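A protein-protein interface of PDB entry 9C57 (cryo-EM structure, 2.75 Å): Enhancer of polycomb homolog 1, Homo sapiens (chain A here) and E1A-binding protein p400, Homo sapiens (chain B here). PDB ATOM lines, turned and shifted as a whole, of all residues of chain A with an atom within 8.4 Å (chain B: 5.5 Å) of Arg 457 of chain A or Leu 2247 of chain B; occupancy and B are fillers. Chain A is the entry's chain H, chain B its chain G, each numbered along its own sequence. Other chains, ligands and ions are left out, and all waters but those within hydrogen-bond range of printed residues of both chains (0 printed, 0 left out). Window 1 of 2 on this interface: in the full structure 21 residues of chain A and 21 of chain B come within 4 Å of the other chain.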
ATOM      1  N   ARG A 437      -9.352  30.553  38.680  1.00  0.00           N
ATOM      2  CA  ARG A 437      -8.465  30.797  37.550  1.00  0.00           C
ATOM      3  C   ARG A 437      -7.394  29.728  37.366  1.00  0.00           C
ATOM      4  O   ARG A 437      -6.952  29.504  36.233  1.00  0.00           O
ATOM      5  CB  ARG A 437      -7.784  32.162  37.704  1.00  0.00           C
ATOM      6  CG  ARG A 437      -7.026  32.632  36.473  1.00  0.00           C
ATOM      7  CD  ARG A 437      -7.957  32.875  35.299  1.00  0.00           C
ATOM      8  NE  ARG A 437      -8.256  31.647  34.572  1.00  0.00           N
ATOM      9  CZ  ARG A 437      -9.145  31.555  33.592  1.00  0.00           C
ATOM     10  NH1 ARG A 437      -9.835  32.606  33.181  1.00  0.00           N
ATOM     11  NH2 ARG A 437      -9.346  30.376  33.009  1.00  0.00           N
ATOM     12  N   ARG A 439      -7.012  26.613  36.840  1.00  0.00           N
ATOM     13  CA  ARG A 439      -7.629  25.377  36.361  1.00  0.00           C
ATOM     14  C   ARG A 439      -6.648  24.577  35.504  1.00  0.00           C
ATOM     15  O   ARG A 439      -6.876  24.311  34.324  1.00  0.00           O
ATOM     16  CB  ARG A 439      -8.914  25.686  35.595  1.00  0.00           C
ATOM     17  CG  ARG A 439      -8.770  26.701  34.473  1.00  0.00           C
ATOM     18  CD  ARG A 439     -10.132  27.144  33.961  1.00  0.00           C
ATOM     19  NE  ARG A 439     -10.838  27.986  34.921  1.00  0.00           N
ATOM     20  CZ  ARG A 439     -12.007  28.567  34.690  1.00  0.00           C
ATOM     21  NH1 ARG A 439     -12.632  28.430  33.532  1.00  0.00           N
ATOM     22  NH2 ARG A 439     -12.564  29.305  35.646  1.00  0.00           N
ATOM     23  N   TYR A 440      -5.533  24.195  36.122  1.00  0.00           N
ATOM     24  CA  TYR A 440      -4.651  23.212  35.518  1.00  0.00           C
ATOM     25  C   TYR A 440      -5.342  21.853  35.484  1.00  0.00           C
ATOM     26  O   TYR A 440      -6.230  21.558  36.287  1.00  0.00           O
ATOM     27  CB  TYR A 440      -3.342  23.106  36.298  1.00  0.00           C
ATOM     28  CG  TYR A 440      -2.451  24.322  36.209  1.00  0.00           C
ATOM     29  CD1 TYR A 440      -2.756  25.482  36.902  1.00  0.00           C
ATOM     30  CD2 TYR A 440      -1.288  24.299  35.454  1.00  0.00           C
ATOM     31  CE1 TYR A 440      -1.938  26.592  36.831  1.00  0.00           C
ATOM     32  CE2 TYR A 440      -0.465  25.402  35.378  1.00  0.00           C
ATOM     33  CZ  TYR A 440      -0.794  26.546  36.069  1.00  0.00           C
ATOM     34  OH  TYR A 440       0.024  27.648  35.996  1.00  0.00           O
ATOM     35  N   CYS A 441      -4.926  21.014  34.540  1.00  0.00           N
ATOM     36  CA  CYS A 441      -5.544  19.704  34.395  1.00  0.00           C
ATOM     37  C   CYS A 441      -4.556  18.751  33.742  1.00  0.00           C
ATOM     38  O   CYS A 441      -3.602  19.169  33.083  1.00  0.00           O
ATOM     39  CB  CYS A 441      -6.832  19.787  33.572  1.00  0.00           C
ATOM     40  SG  CYS A 441      -6.731  20.894  32.146  1.00  0.00           S
ATOM     41  N   THR A 443      -3.179  16.543  30.957  1.00  0.00           N
ATOM     42  CA  THR A 443      -3.254  16.655  29.510  1.00  0.00           C
ATOM     43  C   THR A 443      -2.241  15.719  28.871  1.00  0.00           C
ATOM     44  O   THR A 443      -1.209  15.393  29.465  1.00  0.00           O
ATOM     45  CB  THR A 443      -3.000  18.091  29.031  1.00  0.00           C
ATOM     46  OG1 THR A 443      -1.625  18.432  29.237  1.00  0.00           O
ATOM     47  CG2 THR A 443      -3.884  19.074  29.778  1.00  0.00           C
ATOM     48  N   LEU A 445      -0.224  15.261  25.110  1.00  0.00           N
ATOM     49  CA  LEU A 445       0.092  15.762  23.785  1.00  0.00           C
ATOM     50  C   LEU A 445      -0.038  14.635  22.764  1.00  0.00           C
ATOM     51  O   LEU A 445      -0.251  13.470  23.108  1.00  0.00           O
ATOM     52  CB  LEU A 445       1.501  16.352  23.761  1.00  0.00           C
ATOM     53  CG  LEU A 445       1.780  17.559  24.663  1.00  0.00           C
ATOM     54  CD1 LEU A 445       0.628  18.551  24.633  1.00  0.00           C
ATOM     55  CD2 LEU A 445       2.075  17.129  26.090  1.00  0.00           C
ATOM     56  N   PHE A 454      -0.365  18.302  35.132  1.00  0.00           N
ATOM     57  CA  PHE A 454      -1.181  19.505  35.226  1.00  0.00           C
ATOM     58  C   PHE A 454      -0.660  20.557  34.256  1.00  0.00           C
ATOM     59  O   PHE A 454       0.455  21.063  34.416  1.00  0.00           O
ATOM     60  CB  PHE A 454      -1.175  20.043  36.657  1.00  0.00           C
ATOM     61  CG  PHE A 454      -2.336  19.575  37.507  1.00  0.00           C
ATOM     62  CD1 PHE A 454      -3.173  18.551  37.091  1.00  0.00           C
ATOM     63  CD2 PHE A 454      -2.580  20.167  38.736  1.00  0.00           C
ATOM     64  CE1 PHE A 454      -4.229  18.135  37.878  1.00  0.00           C
ATOM     65  CE2 PHE A 454      -3.634  19.755  39.526  1.00  0.00           C
ATOM     66  CZ  PHE A 454      -4.459  18.737  39.097  1.00  0.00           C
ATOM     67  N   ALA A 455      -1.470  20.883  33.253  1.00  0.00           N
ATOM     68  CA  ALA A 455      -1.126  21.907  32.281  1.00  0.00           C
ATOM     69  C   ALA A 455      -2.406  22.575  31.807  1.00  0.00           C
ATOM     70  O   ALA A 455      -3.434  21.919  31.632  1.00  0.00           O
ATOM     71  CB  ALA A 455      -0.358  21.317  31.093  1.00  0.00           C
ATOM     72  N   ARG A 456      -2.335  23.888  31.600  1.00  0.00           N
ATOM     73  CA  ARG A 456      -3.471  24.659  31.119  1.00  0.00           C
ATOM     74  C   ARG A 456      -3.031  25.530  29.953  1.00  0.00           C
ATOM     75  O   ARG A 456      -1.858  25.890  29.832  1.00  0.00           O
ATOM     76  CB  ARG A 456      -4.078  25.527  32.228  1.00  0.00           C
ATOM     77  CG  ARG A 456      -3.112  26.496  32.873  1.00  0.00           C
ATOM     78  CD  ARG A 456      -3.273  27.889  32.304  1.00  0.00           C
ATOM     79  NE  ARG A 456      -2.452  28.859  33.017  1.00  0.00           N
ATOM     80  CZ  ARG A 456      -2.854  29.553  34.073  1.00  0.00           C
ATOM     81  NH1 ARG A 456      -4.066  29.401  34.582  1.00  0.00           N
ATOM     82  NH2 ARG A 456      -2.016  30.417  34.636  1.00  0.00           N
ATOM     83  N   ARG A 457      -3.986  25.866  29.095  1.00  0.00           N
ATOM     84  CA  ARG A 457      -3.694  26.508  27.824  1.00  0.00           C
ATOM     85  C   ARG A 457      -3.891  28.013  27.936  1.00  0.00           C
ATOM     86  O   ARG A 457      -4.760  28.494  28.666  1.00  0.00           O
ATOM     87  CB  ARG A 457      -4.581  25.950  26.710  1.00  0.00           C
ATOM     88  CG  ARG A 457      -4.985  24.495  26.892  1.00  0.00           C
ATOM     89  CD  ARG A 457      -6.147  24.134  25.993  1.00  0.00           C
ATOM     90  NE  ARG A 457      -5.728  23.668  24.677  1.00  0.00           N
ATOM     91  CZ  ARG A 457      -5.576  24.444  23.614  1.00  0.00           C
ATOM     92  NH1 ARG A 457      -5.660  25.760  23.700  1.00  0.00           N
ATOM     93  NH2 ARG A 457      -5.312  23.884  22.437  1.00  0.00           N
ATOM     94  N   ARG A 458      -3.079  28.751  27.187  1.00  0.00           N
ATOM     95  CA  ARG A 458      -3.050  30.200  27.276  1.00  0.00           C
ATOM     96  C   ARG A 458      -2.598  30.767  25.940  1.00  0.00           C
ATOM     97  O   ARG A 458      -1.912  30.094  25.168  1.00  0.00           O
ATOM     98  CB  ARG A 458      -2.113  30.650  28.400  1.00  0.00           C
ATOM     99  CG  ARG A 458      -2.178  32.119  28.738  1.00  0.00           C
ATOM    100  CD  ARG A 458      -1.309  32.420  29.943  1.00  0.00           C
ATOM    101  NE  ARG A 458       0.106  32.203  29.667  1.00  0.00           N
ATOM    102  CZ  ARG A 458       0.856  33.004  28.923  1.00  0.00           C
ATOM    103  NH1 ARG A 458       0.353  34.081  28.342  1.00  0.00           N
ATOM    104  NH2 ARG A 458       2.144  32.720  28.759  1.00  0.00           N
ATOM    105  N   VAL A 459      -2.986  32.011  25.675  1.00  0.00           N
ATOM    106  CA  VAL A 459      -2.573  32.724  24.471  1.00  0.00           C
ATOM    107  C   VAL A 459      -1.639  33.845  24.893  1.00  0.00           C
ATOM    108  O   VAL A 459      -2.059  34.793  25.568  1.00  0.00           O
ATOM    109  CB  VAL A 459      -3.768  33.288  23.690  1.00  0.00           C
ATOM    110  CG1 VAL A 459      -3.289  33.908  22.387  1.00  0.00           C
ATOM    111  CG2 VAL A 459      -4.811  32.219  23.435  1.00  0.00           C
ATOM    112  N   GLY A 460      -0.377  33.741  24.493  1.00  0.00           N
ATOM    113  CA  GLY A 460       0.589  34.794  24.712  1.00  0.00           C
ATOM    114  C   GLY A 460       0.497  35.855  23.636  1.00  0.00           C
ATOM    115  O   GLY A 460      -0.430  35.889  22.826  1.00  0.00           O
ATOM    116  N   ARG A 464      -0.113  32.934  20.036  1.00  0.00           N
ATOM    117  CA  ARG A 464       0.510  31.621  20.119  1.00  0.00           C
ATOM    118  C   ARG A 464      -0.007  30.905  21.356  1.00  0.00           C
ATOM    119  O   ARG A 464       0.105  31.423  22.472  1.00  0.00           O
ATOM    120  CB  ARG A 464       2.033  31.745  20.161  1.00  0.00           C
ATOM    121  CG  ARG A 464       2.579  32.766  19.175  1.00  0.00           C
ATOM    122  CD  ARG A 464       3.842  32.280  18.498  1.00  0.00           C
ATOM    123  NE  ARG A 464       4.935  32.104  19.446  1.00  0.00           N
ATOM    124  CZ  ARG A 464       5.701  31.025  19.534  1.00  0.00           C
ATOM    125  NH1 ARG A 464       5.522  29.975  18.748  1.00  0.00           N
ATOM    126  NH2 ARG A 464       6.675  30.996  20.438  1.00  0.00           N
ATOM    127  N   VAL A 465      -0.567  29.718  21.157  1.00  0.00           N
ATOM    128  CA  VAL A 465      -1.216  28.973  22.229  1.00  0.00           C
ATOM    129  C   VAL A 465      -0.155  28.198  22.998  1.00  0.00           C
ATOM    130  O   VAL A 465       0.503  27.306  22.452  1.00  0.00           O
ATOM    131  CB  VAL A 465      -2.305  28.042  21.673  1.00  0.00           C
ATOM    132  CG1 VAL A 465      -1.696  26.960  20.809  1.00  0.00           C
ATOM    133  CG2 VAL A 465      -3.102  27.425  22.801  1.00  0.00           C
ATOM    134  N   LEU A 466       0.008  28.534  24.272  1.00  0.00           N
ATOM    135  CA  LEU A 466       1.037  27.956  25.117  1.00  0.00           C
ATOM    136  C   LEU A 466       0.399  27.105  26.205  1.00  0.00           C
ATOM    137  O   LEU A 466      -0.649  27.455  26.754  1.00  0.00           O
ATOM    138  CB  LEU A 466       1.903  29.045  25.767  1.00  0.00           C
ATOM    139  CG  LEU A 466       2.129  30.327  24.963  1.00  0.00           C
ATOM    140  CD1 LEU A 466       2.959  31.321  25.752  1.00  0.00           C
ATOM    141  CD2 LEU A 466       2.794  30.026  23.638  1.00  0.00           C
ATOM    142  N   LEU A 467       1.042  25.985  26.511  1.00  0.00           N
ATOM    143  CA  LEU A 467       0.670  25.153  27.645  1.00  0.00           C
ATOM    144  C   LEU A 467       1.558  25.493  28.833  1.00  0.00           C
ATOM    145  O   LEU A 467       2.783  25.368  28.757  1.00  0.00           O
ATOM    146  CB  LEU A 467       0.794  23.666  27.309  1.00  0.00           C
ATOM    147  CG  LEU A 467      -0.348  22.958  26.573  1.00  0.00           C
ATOM    148  CD1 LEU A 467      -1.656  23.114  27.330  1.00  0.00           C
ATOM    149  CD2 LEU A 467      -0.498  23.439  25.146  1.00  0.00           C
ATOM    150  N   ASP A 468       0.936  25.925  29.923  1.00  0.00           N
ATOM    151  CA  ASP A 468       1.605  26.109  31.200  1.00  0.00           C
ATOM    152  C   ASP A 468       1.692  24.763  31.905  1.00  0.00           C
ATOM    153  O   ASP A 468       1.118  23.770  31.454  1.00  0.00           O
ATOM    154  CB  ASP A 468       0.847  27.116  32.061  1.00  0.00           C
ATOM    155  CG  ASP A 468       1.760  28.095  32.746  1.00  0.00           C
ATOM    156  OD1 ASP A 468       2.537  27.675  33.627  1.00  0.00           O
ATOM    157  OD2 ASP A 468       1.698  29.289  32.394  1.00  0.00           O
ATOM    158  N   ARG A 469       2.416  24.725  33.021  1.00  0.00           N
ATOM    159  CA  ARG A 469       2.612  23.460  33.714  1.00  0.00           C
ATOM    160  C   ARG A 469       2.791  23.663  35.210  1.00  0.00           C
ATOM    161  O   ARG A 469       3.138  24.750  35.679  1.00  0.00           O
ATOM    162  CB  ARG A 469       3.820  22.707  33.160  1.00  0.00           C
ATOM    163  CG  ARG A 469       3.623  22.195  31.751  1.00  0.00           C
ATOM    164  CD  ARG A 469       4.824  21.404  31.302  1.00  0.00           C
ATOM    165  NE  ARG A 469       5.996  22.257  31.170  1.00  0.00           N
ATOM    166  CZ  ARG A 469       7.206  21.821  30.858  1.00  0.00           C
ATOM    167  NH1 ARG A 469       7.441  20.541  30.624  1.00  0.00           N
ATOM    168  NH2 ARG A 469       8.204  22.693  30.771  1.00  0.00           N
ATOM    169  N   ALA B2228      -1.393  22.018  18.810  1.00  0.00           N
ATOM    170  CA  ALA B2228      -1.490  23.258  19.566  1.00  0.00           C
ATOM    171  C   ALA B2228      -2.787  24.000  19.300  1.00  0.00           C
ATOM    172  O   ALA B2228      -3.379  24.559  20.231  1.00  0.00           O
ATOM    173  CB  ALA B2228      -0.302  24.164  19.220  1.00  0.00           C
ATOM    174  N   TYR B2229      -3.246  24.018  18.053  1.00  0.00           N
ATOM    175  CA  TYR B2229      -4.417  24.780  17.654  1.00  0.00           C
ATOM    176  C   TYR B2229      -5.566  23.896  17.188  1.00  0.00           C
ATOM    177  O   TYR B2229      -6.367  24.332  16.356  1.00  0.00           O
ATOM    178  CB  TYR B2229      -4.040  25.762  16.545  1.00  0.00           C
ATOM    179  CG  TYR B2229      -2.854  26.647  16.866  1.00  0.00           C
ATOM    180  CD1 TYR B2229      -1.560  26.213  16.634  1.00  0.00           C
ATOM    181  CD2 TYR B2229      -3.031  27.920  17.383  1.00  0.00           C
ATOM    182  CE1 TYR B2229      -0.476  27.017  16.918  1.00  0.00           C
ATOM    183  CE2 TYR B2229      -1.951  28.733  17.667  1.00  0.00           C
ATOM    184  CZ  TYR B2229      -0.678  28.275  17.432  1.00  0.00           C
ATOM    185  OH  TYR B2229       0.402  29.076  17.713  1.00  0.00           O
ATOM    186  N   SER B2230      -5.667  22.666  17.695  1.00  0.00           N
ATOM    187  CA  SER B2230      -6.728  21.746  17.298  1.00  0.00           C
ATOM    188  C   SER B2230      -7.336  21.041  18.507  1.00  0.00           C
ATOM    189  O   SER B2230      -7.914  19.960  18.380  1.00  0.00           O
ATOM    190  CB  SER B2230      -6.208  20.729  16.285  1.00  0.00           C
ATOM    191  OG  SER B2230      -5.757  21.382  15.110  1.00  0.00           O
ATOM    192  N   MET B2231      -7.181  21.637  19.689  1.00  0.00           N
ATOM    193  CA  MET B2231      -7.867  21.263  20.926  1.00  0.00           C
ATOM    194  C   MET B2231      -7.349  19.961  21.529  1.00  0.00           C
ATOM    195  O   MET B2231      -7.472  19.751  22.740  1.00  0.00           O
ATOM    196  CB  MET B2231      -9.384  21.205  20.641  1.00  0.00           C
ATOM    197  CG  MET B2231     -10.325  20.545  21.669  1.00  0.00           C
ATOM    198  SD  MET B2231     -10.057  18.823  22.157  1.00  0.00           S
ATOM    199  CE  MET B2231      -9.779  18.031  20.574  1.00  0.00           C
ATOM    200  N   GLU B2232      -6.740  19.098  20.721  1.00  0.00           N
ATOM    201  CA  GLU B2232      -5.727  18.140  21.152  1.00  0.00           C
ATOM    202  C   GLU B2232      -6.143  17.171  22.259  1.00  0.00           C
ATOM    203  O   GLU B2232      -5.484  16.141  22.440  1.00  0.00           O
ATOM    204  CB  GLU B2232      -4.484  18.896  21.624  1.00  0.00           C
ATOM    205  CG  GLU B2232      -4.218  20.203  20.896  1.00  0.00           C
ATOM    206  CD  GLU B2232      -4.268  20.061  19.387  1.00  0.00           C
ATOM    207  OE1 GLU B2232      -4.216  18.919  18.887  1.00  0.00           O
ATOM    208  OE2 GLU B2232      -4.348  21.097  18.698  1.00  0.00           O
ATOM    209  N   VAL B2244     -13.367  21.252  27.226  1.00  0.00           N
ATOM    210  CA  VAL B2244     -12.416  21.481  26.146  1.00  0.00           C
ATOM    211  C   VAL B2244     -11.149  22.097  26.717  1.00  0.00           C
ATOM    212  O   VAL B2244     -10.374  22.726  25.987  1.00  0.00           O
ATOM    213  CB  VAL B2244     -13.029  22.385  25.061  1.00  0.00           C
ATOM    214  CG1 VAL B2244     -13.011  23.843  25.503  1.00  0.00           C
ATOM    215  CG2 VAL B2244     -12.297  22.212  23.742  1.00  0.00           C
ATOM    216  N   MET B2245     -10.924  21.913  28.025  1.00  0.00           N
ATOM    217  CA  MET B2245      -9.838  22.576  28.739  1.00  0.00           C
ATOM    218  C   MET B2245      -9.729  23.995  28.199  1.00  0.00           C
ATOM    219  O   MET B2245      -8.769  24.327  27.493  1.00  0.00           O
ATOM    220  CB  MET B2245      -8.518  21.806  28.605  1.00  0.00           C
ATOM    221  CG  MET B2245      -8.197  21.269  27.218  1.00  0.00           C
ATOM    222  SD  MET B2245      -6.529  20.583  27.139  1.00  0.00           S
ATOM    223  CE  MET B2245      -6.383  20.207  25.396  1.00  0.00           C
ATOM    224  N   PRO B2246     -10.698  24.852  28.508  1.00  0.00           N
ATOM    225  CA  PRO B2246     -10.893  26.075  27.722  1.00  0.00           C
ATOM    226  C   PRO B2246      -9.660  26.960  27.726  1.00  0.00           C
ATOM    227  O   PRO B2246      -8.696  26.758  28.465  1.00  0.00           O
ATOM    228  CB  PRO B2246     -12.078  26.758  28.410  1.00  0.00           C
ATOM    229  CG  PRO B2246     -12.063  26.231  29.801  1.00  0.00           C
ATOM    230  CD  PRO B2246     -11.551  24.825  29.707  1.00  0.00           C
ATOM    231  N   LEU B2247      -9.711  27.963  26.863  1.00  0.00           N
ATOM    232  CA  LEU B2247      -8.592  28.867  26.686  1.00  0.00           C
ATOM    233  C   LEU B2247      -8.540  29.886  27.817  1.00  0.00           C
ATOM    234  O   LEU B2247      -9.528  30.121  28.518  1.00  0.00           O
ATOM    235  CB  LEU B2247      -8.708  29.613  25.361  1.00  0.00           C
ATOM    236  CG  LEU B2247      -7.825  29.113  24.227  1.00  0.00           C
ATOM    237  CD1 LEU B2247      -6.399  29.573  24.458  1.00  0.00           C
ATOM    238  CD2 LEU B2247      -7.934  27.621  24.056  1.00  0.00           C
ATOM    239  N   TRP B2248      -7.365  30.486  27.996  1.00  0.00           N
ATOM    240  CA  TRP B2248      -7.249  31.755  28.710  1.00  0.00           C
ATOM    241  C   TRP B2248      -6.769  32.773  27.680  1.00  0.00           C
ATOM    242  O   TRP B2248      -5.578  33.043  27.529  1.00  0.00           O
ATOM    243  CB  TRP B2248      -6.308  31.645  29.909  1.00  0.00           C
ATOM    244  CG  TRP B2248      -6.126  32.947  30.657  1.00  0.00           C
ATOM    245  CD1 TRP B2248      -6.723  34.142  30.382  1.00  0.00           C
ATOM    246  CD2 TRP B2248      -5.291  33.175  31.800  1.00  0.00           C
ATOM    247  NE1 TRP B2248      -6.313  35.097  31.274  1.00  0.00           N
ATOM    248  CE2 TRP B2248      -5.435  34.529  32.158  1.00  0.00           C
ATOM    249  CE3 TRP B2248      -4.438  32.367  32.554  1.00  0.00           C
ATOM    250  CZ2 TRP B2248      -4.756  35.094  33.232  1.00  0.00           C
ATOM    251  CZ3 TRP B2248      -3.765  32.930  33.623  1.00  0.00           C
ATOM    252  CH2 TRP B2248      -3.928  34.280  33.951  1.00  0.00           C
ATOM    253  N   THR B2249      -7.726  33.342  26.962  1.00  0.00           N
ATOM    254  CA  THR B2249      -7.437  34.314  25.922  1.00  0.00           C
ATOM    255  C   THR B2249      -7.283  35.697  26.534  1.00  0.00           C
ATOM    256  O   THR B2249      -7.502  35.895  27.729  1.00  0.00           O
ATOM    257  CB  THR B2249      -8.555  34.327  24.878  1.00  0.00           C
ATOM    258  OG1 THR B2249      -9.574  35.251  25.281  1.00  0.00           O
ATOM    259  CG2 THR B2249      -9.161  32.948  24.677  1.00  0.00           C
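Printed residues of chain B that touch a printed residue of chain A: Ala 2228, Tyr 2229, Met 2231, Met 2245, Leu 2247 and Trp 2248. Hydrophobic or aromatic side chains of chain B that line the printed part of chain A: Ala 2228, Tyr 2229, Met 2245, Leu 2247 and Trp 2248. Along chain B the printed residues that touch a printed residue of chain A span positions 2228 to 2248. Among the printed residues, 12 pairs touch across the chains. Among the printed residues, no Asp or Glu carboxylate lies within 4 Å of a Lys or Arg side-chain nitrogen of the other chain.
Of the printed residues of chain B, Arg 457 of chain A touches Ala 2228 (3.0 Å), Met 2231 (3.96 Å), Met 2245 (3.0 Å), Leu 2247 (3.0 Å) and Trp 2248 (3.3 Å). Gly 460 of chain A touches none of the printed residues of chain B. Of the printed residues of chain B, Arg 464 of chain A touches Tyr 2229 (3.5 Å). Of the printed residues of chain B, Val 465 of chain A touches Ala 2228 and Tyr 2229. Asp 468 of chain A touches none of the printed residues of chain B. Printed residues of chain A within 4 Å of Ala 2228 of chain B: Arg 457 and Val 465. Printed residues of chain A within 4 Å of Met 2245 of chain B: Arg 457 (3.0 Å). Leu 2247 of chain B touches two residues of chain A. The nearest residue of chain B that does not touch Arg 457 of chain A is Glu 2232 of chain B (4.1 Å). The nearest printed residue of chain A that does not touch Leu 2247 of chain B is Arg 458 of chain A (4.3 Å).
O of Arg 456 of chain A lies within hydrogen-bond range of N of Asp 468 of chain A (2.8 Å). OE2 of Glu 2232 of chain B lies within hydrogen-bond range of N of Tyr 2229 of chain B (3.2 Å). N of Leu 466 of chain A sits at hydrogen-bond distance from O of Arg 458 of chain A (2.6 Å). The side-chain carboxylate (OE2) of Glu 2232 of chain B sits at hydrogen-bond distance from the backbone NH (N) of Ala 2228 of chain B (3.1 Å). O of Arg 437 of chain A is in hydrogen-bond range of NH1 of Arg 456 of chain A.
The backbone carbonyl oxygen of Ala 2228 of chain B sits at hydrogen-bond distance from the guanidinium group of Arg 457 of chain A (3.0 Å). The backbone NH (N) of Trp 2248 of chain B sits at hydrogen-bond distance from the backbone carbonyl oxygen (O) of Arg 457 of chain A (3.3 Å). N of Val 459 of chain A lies within hydrogen-bond range of O of Trp 2248 of chain B, 3.3 Å away.
Among the printed residues, pairs that only touch across the chains: Arg 456 of chain A with Trp 2248 of chain B, Arg 457 of chain A with Met 2231 of chain B, Arg 457 of chain A with Met 2245 of chain B, Arg 457 of chain A with Leu 2247 of chain B, Arg 458 of chain A with Trp 2248 of chain B, Val 459 of chain A with Leu 2247 of chain B, Arg 464 of chain A with Tyr 2229 of chain B, Val 465 of chain A with Ala 2228 of chain B and Val 465 of chain A with Tyr 2229 of chain B.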
